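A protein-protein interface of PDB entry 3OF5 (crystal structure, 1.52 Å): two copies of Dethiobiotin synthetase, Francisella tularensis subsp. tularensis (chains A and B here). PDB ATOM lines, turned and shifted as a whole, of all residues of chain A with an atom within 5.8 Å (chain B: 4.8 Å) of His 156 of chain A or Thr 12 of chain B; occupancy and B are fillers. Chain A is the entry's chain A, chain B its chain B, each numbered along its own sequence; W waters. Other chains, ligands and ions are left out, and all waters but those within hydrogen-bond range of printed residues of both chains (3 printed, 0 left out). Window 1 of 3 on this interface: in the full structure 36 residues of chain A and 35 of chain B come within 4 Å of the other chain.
The backbone carbonyl oxygen (O) of Thr 12 of chain B sits at hydrogen-bond distance from a ring nitrogen (NE2) of His 156 of chain A (2.9 Å). The backbone carbonyl oxygen (O) of Thr 12 of chain A lies within hydrogen-bond range of a ring nitrogen (NE2) of His 156 of chain B, at 2.9 Å.
The backbone NH (N) of Thr 12 of chain B lies within hydrogen-bond range of the backbone carbonyl oxygen (O) of Val 146 of chain B (3.1 Å). OG1 of Thr 160 of chain A lies within hydrogen-bond range of O of His 156 of chain A, at 2.8 Å. The backbone carbonyl oxygen (O) of His 156 of chain B lies within hydrogen-bond range of the side-chain hydroxyl (OG1) of Thr 160 of chain B (2.9 Å).
Among the printed residues, merely in contact across the chains: Asp 13 of chain A with His 156 of chain B (3.1 Å), His 156 of chain A with Asp 13 of chain B (3.0 Å), His 156 of chain A with His 156 of chain B (3.3 Å) and Leu 159 of chain A with Thr 160 of chain B (3.7 Å).
Of the printed residues of chain B, His 156 of chain A touches Thr 12, Asp 13 and His 156. Printed residues of chain B within 4 Å of Asp 13 of chain A: His 156 (3.1 Å). Printed residues of chain B within 4 Å of Thr 12 of chain A: His 156. Printed residues of chain A within 4 Å of Thr 160 of chain B: Leu 159 (3.7 Å). Of the printed residues of chain A, Asp 13 of chain B touches His 156. The nearest printed residue of chain B that does not touch His 156 of chain A is Thr 160 of chain B (6.2 Å). The nearest printed residue of chain B that does not touch Leu 159 of chain A is His 156 of chain B (4.9 Å).
Hydrophobic or aromatic side chains of chain A that line the printed part of chain B: His 156 and Leu 159. Along chain A the printed residues that touch a printed residue of chain B span positions 12 to 159. Of the 12 printed residues of chain B, 4 touch a printed residue of chain A. Printed residues of chain B that touch a printed residue of chain A: Thr 12, Asp 13, His 156 and Thr 160. Hydrophobic or aromatic side chains of chain B within 4 Å of the printed part of chain A: His 156. Among the printed residues, no Asp or Glu carboxylate lies within 4 Å of a Lys or Arg side-chain nitrogen of the other chain.
Thr 12 of chain A touches His 156 of chain B, and with the chains exchanged His 156 of chain A touches Thr 12 of chain B. Asp 13 of chain A touches His 156 of chain B, and with the chains exchanged His 156 of chain A touches Asp 13 of chain B. His 156 of chain B touches its own counterpart, His 156 of chain A. Of the 6 pairs that touch across the chains among the printed residues, 5 have their exchanged pair printed and touching as well.
Water W3 lies within hydrogen-bond range of O of Gly 11 of chain B (2.8 Å), OG1 of Thr 160 of chain B (3.0 Å) and ND2 of Asn 155 of chain A (3.1 Å). Water W2 lies within hydrogen-bond range of the backbone carbonyl oxygen of Gly 152 of chain A (2.8 Å), the side-chain carboxylate of Asp 13 of chain B (3.0 Å), the side-chain amide nitrogen of Asn 155 of chain A (3.0 Å) and a ring nitrogen (NE2) of His 156 of chain A (3.2 Å). Water W1 bridges the side-chain carboxylate (OD1) of Asp 13 of chain A and a ring nitrogen (NE2) of His 156 of chain B.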
ATOM      1  N   THR A  12     -12.308  18.425  -5.330  1.00  0.00           N
ATOM      2  CA  THR A  12     -12.584  19.664  -4.598  1.00  0.00           C
ATOM      3  C   THR A  12     -12.744  19.397  -3.110  1.00  0.00           C
ATOM      4  O   THR A  12     -12.742  20.339  -2.314  1.00  0.00           O
ATOM      5  CB  THR A  12     -13.830  20.329  -5.159  1.00  0.00           C
ATOM      6  OG1 THR A  12     -14.878  19.363  -5.169  1.00  0.00           O
ATOM      7  CG2 THR A  12     -13.577  20.891  -6.537  1.00  0.00           C
ATOM      8  N   ASP A  13     -12.880  18.119  -2.743  1.00  0.00           N
ATOM      9  CA  ASP A  13     -12.985  17.618  -1.359  1.00  0.00           C
ATOM     10  C   ASP A  13     -12.561  16.138  -1.343  1.00  0.00           C
ATOM     11  O   ASP A  13     -12.296  15.606  -2.413  1.00  0.00           O
ATOM     12  CB  ASP A  13     -14.397  17.798  -0.818  1.00  0.00           C
ATOM     13  CG  ASP A  13     -14.502  17.837   0.716  1.00  0.00           C
ATOM     14  OD1 ASP A  13     -13.455  17.623   1.406  1.00  0.00           O
ATOM     15  OD2 ASP A  13     -15.587  18.111   1.212  1.00  0.00           O
ATOM     16  N   GLY A 152     -21.879  24.405  -1.331  1.00  0.00           N
ATOM     17  CA  GLY A 152     -20.516  24.684  -0.912  1.00  0.00           C
ATOM     18  C   GLY A 152     -19.502  24.378  -1.992  1.00  0.00           C
ATOM     19  O   GLY A 152     -18.337  24.802  -1.895  1.00  0.00           O
ATOM     20  N   CYS A 153     -19.940  23.656  -3.046  1.00  0.00           N
ATOM     21  CA  CYS A 153     -19.022  23.279  -4.116  1.00  0.00           C
ATOM     22  C   CYS A 153     -18.470  24.456  -4.869  1.00  0.00           C
ATOM     23  O   CYS A 153     -17.371  24.334  -5.423  1.00  0.00           O
ATOM     24  CB  CYS A 153     -19.619  22.247  -5.066  1.00  0.00           C
ATOM     25  SG  CYS A 153     -20.842  22.916  -6.232  1.00  0.00           S
ATOM     26  N   ILE A 154     -19.210  25.581  -4.945  1.00  0.00           N
ATOM     27  CA  ILE A 154     -18.695  26.699  -5.717  1.00  0.00           C
ATOM     28  C   ILE A 154     -17.450  27.256  -5.046  1.00  0.00           C
ATOM     29  O   ILE A 154     -16.401  27.380  -5.692  1.00  0.00           O
ATOM     30  CB  ILE A 154     -19.765  27.776  -5.974  1.00  0.00           C
ATOM     31  CG1 ILE A 154     -20.970  27.103  -6.688  1.00  0.00           C
ATOM     32  CG2 ILE A 154     -19.158  28.882  -6.859  1.00  0.00           C
ATOM     33  CD1 ILE A 154     -22.274  27.958  -6.641  1.00  0.00           C
ATOM     34  N   ASN A 155     -17.561  27.563  -3.755  1.00  0.00           N
ATOM     35  CA  ASN A 155     -16.410  28.043  -3.006  1.00  0.00           C
ATOM     36  C   ASN A 155     -15.196  27.088  -3.177  1.00  0.00           C
ATOM     37  O   ASN A 155     -14.088  27.520  -3.536  1.00  0.00           O
ATOM     38  CB  ASN A 155     -16.802  28.134  -1.538  1.00  0.00           C
ATOM     39  CG  ASN A 155     -15.648  28.499  -0.664  1.00  0.00           C
ATOM     40  OD1 ASN A 155     -14.923  29.478  -0.910  1.00  0.00           O
ATOM     41  ND2 ASN A 155     -15.496  27.772   0.452  1.00  0.00           N
ATOM     42  N   HIS A 156     -15.413  25.783  -2.988  1.00  0.00           N
ATOM     43  CA  HIS A 156     -14.291  24.852  -3.076  1.00  0.00           C
ATOM     44  C   HIS A 156     -13.696  24.717  -4.456  1.00  0.00           C
ATOM     45  O   HIS A 156     -12.460  24.580  -4.579  1.00  0.00           O
ATOM     46  CB  HIS A 156     -14.737  23.488  -2.584  1.00  0.00           C
ATOM     47  CG  HIS A 156     -14.982  23.476  -1.112  1.00  0.00           C
ATOM     48  ND1 HIS A 156     -15.845  22.573  -0.531  1.00  0.00           N
ATOM     49  CD2 HIS A 156     -14.460  24.278  -0.146  1.00  0.00           C
ATOM     50  CE1 HIS A 156     -15.812  22.842   0.767  1.00  0.00           C
ATOM     51  NE2 HIS A 156     -15.016  23.878   1.044  1.00  0.00           N
ATOM     52  N   THR A 157     -14.545  24.757  -5.500  1.00  0.00           N
ATOM     53  CA  THR A 157     -14.013  24.625  -6.849  1.00  0.00           C
ATOM     54  C   THR A 157     -13.205  25.879  -7.209  1.00  0.00           C
ATOM     55  O   THR A 157     -12.112  25.753  -7.769  1.00  0.00           O
ATOM     56  CB  THR A 157     -15.156  24.413  -7.855  1.00  0.00           C
ATOM     57  OG1 THR A 157     -15.922  23.303  -7.404  1.00  0.00           O
ATOM     58  CG2 THR A 157     -14.647  24.111  -9.268  1.00  0.00           C
ATOM     59  N   LEU A 158     -13.741  27.085  -6.902  1.00  0.00           N
ATOM     60  CA  LEU A 158     -13.027  28.323  -7.222  1.00  0.00           C
ATOM     61  C   LEU A 158     -11.715  28.418  -6.432  1.00  0.00           C
ATOM     62  O   LEU A 158     -10.692  28.850  -6.984  1.00  0.00           O
ATOM     63  CB  LEU A 158     -13.922  29.546  -6.953  1.00  0.00           C
ATOM     64  CG  LEU A 158     -15.200  29.642  -7.768  1.00  0.00           C
ATOM     65  CD1 LEU A 158     -15.945  30.901  -7.396  1.00  0.00           C
ATOM     66  CD2 LEU A 158     -14.888  29.619  -9.278  1.00  0.00           C
ATOM     67  N   LEU A 159     -11.735  28.035  -5.146  1.00  0.00           N
ATOM     68  CA  LEU A 159     -10.506  28.077  -4.354  1.00  0.00           C
ATOM     69  C   LEU A 159      -9.461  27.161  -4.968  1.00  0.00           C
ATOM     70  O   LEU A 159      -8.303  27.553  -5.081  1.00  0.00           O
ATOM     71  CB  LEU A 159     -10.748  27.636  -2.912  1.00  0.00           C
ATOM     72  CG  LEU A 159     -11.451  28.635  -2.013  1.00  0.00           C
ATOM     73  CD1 LEU A 159     -11.887  27.963  -0.716  1.00  0.00           C
ATOM     74  CD2 LEU A 159     -10.551  29.833  -1.677  1.00  0.00           C
ATOM     75  N   THR A 160      -9.871  25.954  -5.390  1.00  0.00           N
ATOM     76  CA  THR A 160      -8.915  25.006  -5.988  1.00  0.00           C
ATOM     77  C   THR A 160      -8.352  25.532  -7.310  1.00  0.00           C
ATOM     78  O   THR A 160      -7.138  25.490  -7.517  1.00  0.00           O
ATOM     79  CB  THR A 160      -9.571  23.625  -6.165  1.00  0.00           C
ATOM     80  OG1 THR A 160     -10.046  23.168  -4.893  1.00  0.00           O
ATOM     81  CG2 THR A 160      -8.619  22.594  -6.760  1.00  0.00           C
ATOM     82  N   ILE A 161      -9.225  26.052  -8.190  1.00  0.00           N
ATOM     83  CA  ILE A 161      -8.748  26.590  -9.466  1.00  0.00           C
ATOM     84  C   ILE A 161      -7.797  27.741  -9.223  1.00  0.00           C
ATOM     85  O   ILE A 161      -6.763  27.823  -9.906  1.00  0.00           O
ATOM     86  CB  ILE A 161      -9.945  26.979 -10.372  1.00  0.00           C
ATOM     87  CG1 ILE A 161     -10.693  25.708 -10.809  1.00  0.00           C
ATOM     88  CG2 ILE A 161      -9.491  27.812 -11.609  1.00  0.00           C
ATOM     89  CD1 ILE A 161     -12.039  25.957 -11.531  1.00  0.00           C
ATOM     90  N   ILE B  10     -15.789  33.888   8.469  1.00  0.00           N
ATOM     91  CA  ILE B  10     -16.069  32.991   7.359  1.00  0.00           C
ATOM     92  C   ILE B  10     -15.775  31.575   7.765  1.00  0.00           C
ATOM     93  O   ILE B  10     -15.045  31.353   8.733  1.00  0.00           O
ATOM     94  CB  ILE B  10     -15.266  33.351   6.087  1.00  0.00           C
ATOM     95  CG1 ILE B  10     -13.783  33.252   6.339  1.00  0.00           C
ATOM     96  CG2 ILE B  10     -15.688  34.729   5.486  1.00  0.00           C
ATOM     97  CD1 ILE B  10     -12.894  33.260   5.064  1.00  0.00           C
ATOM     98  N   GLY B  11     -16.349  30.630   7.030  1.00  0.00           N
ATOM     99  CA  GLY B  11     -16.064  29.222   7.251  1.00  0.00           C
ATOM    100  C   GLY B  11     -15.203  28.628   6.158  1.00  0.00           C
ATOM    101  O   GLY B  11     -15.034  29.226   5.087  1.00  0.00           O
ATOM    102  N   THR B  12     -14.685  27.413   6.413  1.00  0.00           N
ATOM    103  CA  THR B  12     -13.909  26.631   5.438  1.00  0.00           C
ATOM    104  C   THR B  12     -14.817  25.867   4.504  1.00  0.00           C
ATOM    105  O   THR B  12     -14.354  25.333   3.492  1.00  0.00           O
ATOM    106  CB  THR B  12     -12.985  25.645   6.143  1.00  0.00           C
ATOM    107  OG1 THR B  12     -13.734  24.932   7.139  1.00  0.00           O
ATOM    108  CG2 THR B  12     -11.826  26.325   6.732  1.00  0.00           C
ATOM    109  N   ASP B  13     -16.104  25.778   4.861  1.00  0.00           N
ATOM    110  CA  ASP B  13     -17.128  25.093   4.068  1.00  0.00           C
ATOM    111  C   ASP B  13     -18.484  25.577   4.545  1.00  0.00           C
ATOM    112  O   ASP B  13     -18.557  26.384   5.462  1.00  0.00           O
ATOM    113  CB  ASP B  13     -17.031  23.567   4.271  1.00  0.00           C
ATOM    114  CG  ASP B  13     -17.780  22.708   3.236  1.00  0.00           C
ATOM    115  OD1 ASP B  13     -18.380  23.292   2.277  1.00  0.00           O
ATOM    116  OD2 ASP B  13     -17.809  21.489   3.403  1.00  0.00           O
ATOM    117  N   VAL B  16     -20.109  24.604   9.017  1.00  0.00           N
ATOM    118  CA  VAL B  16     -18.939  24.364   9.864  1.00  0.00           C
ATOM    119  C   VAL B  16     -19.208  24.834  11.292  1.00  0.00           C
ATOM    120  O   VAL B  16     -18.278  24.901  12.101  1.00  0.00           O
ATOM    121  CB  VAL B  16     -17.607  24.962   9.306  1.00  0.00           C
ATOM    122  CG1 VAL B  16     -17.215  24.311   7.979  1.00  0.00           C
ATOM    123  CG2 VAL B  16     -17.651  26.492   9.202  1.00  0.00           C
ATOM    124  N   LEU B 145     -11.440  32.863  10.613  1.00  0.00           N
ATOM    125  CA  LEU B 145     -11.795  31.681   9.847  1.00  0.00           C
ATOM    126  C   LEU B 145     -12.140  30.537  10.774  1.00  0.00           C
ATOM    127  O   LEU B 145     -11.303  30.113  11.569  1.00  0.00           O
ATOM    128  CB  LEU B 145     -10.610  31.291   8.953  1.00  0.00           C
ATOM    129  CG  LEU B 145     -10.752  29.998   8.177  1.00  0.00           C
ATOM    130  CD1 LEU B 145     -11.928  30.073   7.197  1.00  0.00           C
ATOM    131  CD2 LEU B 145      -9.451  29.676   7.431  1.00  0.00           C
ATOM    132  N   VAL B 146     -13.348  29.989  10.602  1.00  0.00           N
ATOM    133  CA  VAL B 146     -13.853  28.870  11.377  1.00  0.00           C
ATOM    134  C   VAL B 146     -13.653  27.634  10.531  1.00  0.00           C
ATOM    135  O   VAL B 146     -14.204  27.558   9.424  1.00  0.00           O
ATOM    136  CB  VAL B 146     -15.345  29.018  11.755  1.00  0.00           C
ATOM    137  CG1 VAL B 146     -15.837  27.766  12.513  1.00  0.00           C
ATOM    138  CG2 VAL B 146     -15.571  30.291  12.566  1.00  0.00           C
ATOM    139  N   SER B 147     -12.900  26.649  11.054  1.00  0.00           N
ATOM    140  CA  SER B 147     -12.658  25.393  10.358  1.00  0.00           C
ATOM    141  C   SER B 147     -13.292  24.247  11.129  1.00  0.00           C
ATOM    142  O   SER B 147     -12.942  24.049  12.293  1.00  0.00           O
ATOM    143  CB  SER B 147     -11.157  25.163  10.253  1.00  0.00           C
ATOM    144  OG  SER B 147     -10.850  23.890   9.716  1.00  0.00           O
ATOM    145  N   ALA B 148     -14.199  23.469  10.500  1.00  0.00           N
ATOM    146  CA  ALA B 148     -14.769  22.312  11.175  1.00  0.00           C
ATOM    147  C   ALA B 148     -13.773  21.193  10.953  1.00  0.00           C
ATOM    148  O   ALA B 148     -13.356  20.978   9.807  1.00  0.00           O
ATOM    149  CB  ALA B 148     -16.115  21.911  10.589  1.00  0.00           C
ATOM    150  N   HIS B 156      -9.134  22.371   2.800  1.00  0.00           N
ATOM    151  CA  HIS B 156      -9.992  23.541   2.747  1.00  0.00           C
ATOM    152  C   HIS B 156      -9.487  24.714   3.528  1.00  0.00           C
ATOM    153  O   HIS B 156      -9.652  25.859   3.095  1.00  0.00           O
ATOM    154  CB  HIS B 156     -11.398  23.170   3.205  1.00  0.00           C
ATOM    155  CG  HIS B 156     -12.071  22.246   2.241  1.00  0.00           C
ATOM    156  ND1 HIS B 156     -13.042  21.354   2.656  1.00  0.00           N
ATOM    157  CD2 HIS B 156     -11.898  22.112   0.900  1.00  0.00           C
ATOM    158  CE1 HIS B 156     -13.431  20.713   1.563  1.00  0.00           C
ATOM    159  NE2 HIS B 156     -12.757  21.114   0.486  1.00  0.00           N
ATOM    160  N   THR B 157      -8.871  24.456   4.701  1.00  0.00           N
ATOM    161  CA  THR B 157      -8.375  25.558   5.515  1.00  0.00           C
ATOM    162  C   THR B 157      -7.183  26.239   4.818  1.00  0.00           C
ATOM    163  O   THR B 157      -7.137  27.474   4.733  1.00  0.00           O
ATOM    164  CB  THR B 157      -8.010  25.053   6.919  1.00  0.00           C
ATOM    165  OG1 THR B 157      -9.162  24.396   7.467  1.00  0.00           O
ATOM    166  CG2 THR B 157      -7.605  26.183   7.868  1.00  0.00           C
ATOM    167  N   THR B 160      -8.275  28.324   1.796  1.00  0.00           N
ATOM    168  CA  THR B 160      -8.907  29.585   2.204  1.00  0.00           C
ATOM    169  C   THR B 160      -7.830  30.573   2.679  1.00  0.00           C
ATOM    170  O   THR B 160      -7.855  31.731   2.272  1.00  0.00           O
ATOM    171  CB  THR B 160      -9.932  29.340   3.305  1.00  0.00           C
ATOM    172  OG1 THR B 160     -10.934  28.419   2.847  1.00  0.00           O
ATOM    173  CG2 THR B 160     -10.585  30.646   3.751  1.00  0.00           C
HETATM  174  O   HOH W   1     -10.706  18.645   1.102  1.00  0.00           O
HETATM  175  O   HOH W   2     -17.658  25.699   0.720  1.00  0.00           O
HETATM  176  O   HOH W   3     -13.758  29.251   2.605  1.00  0.00           O
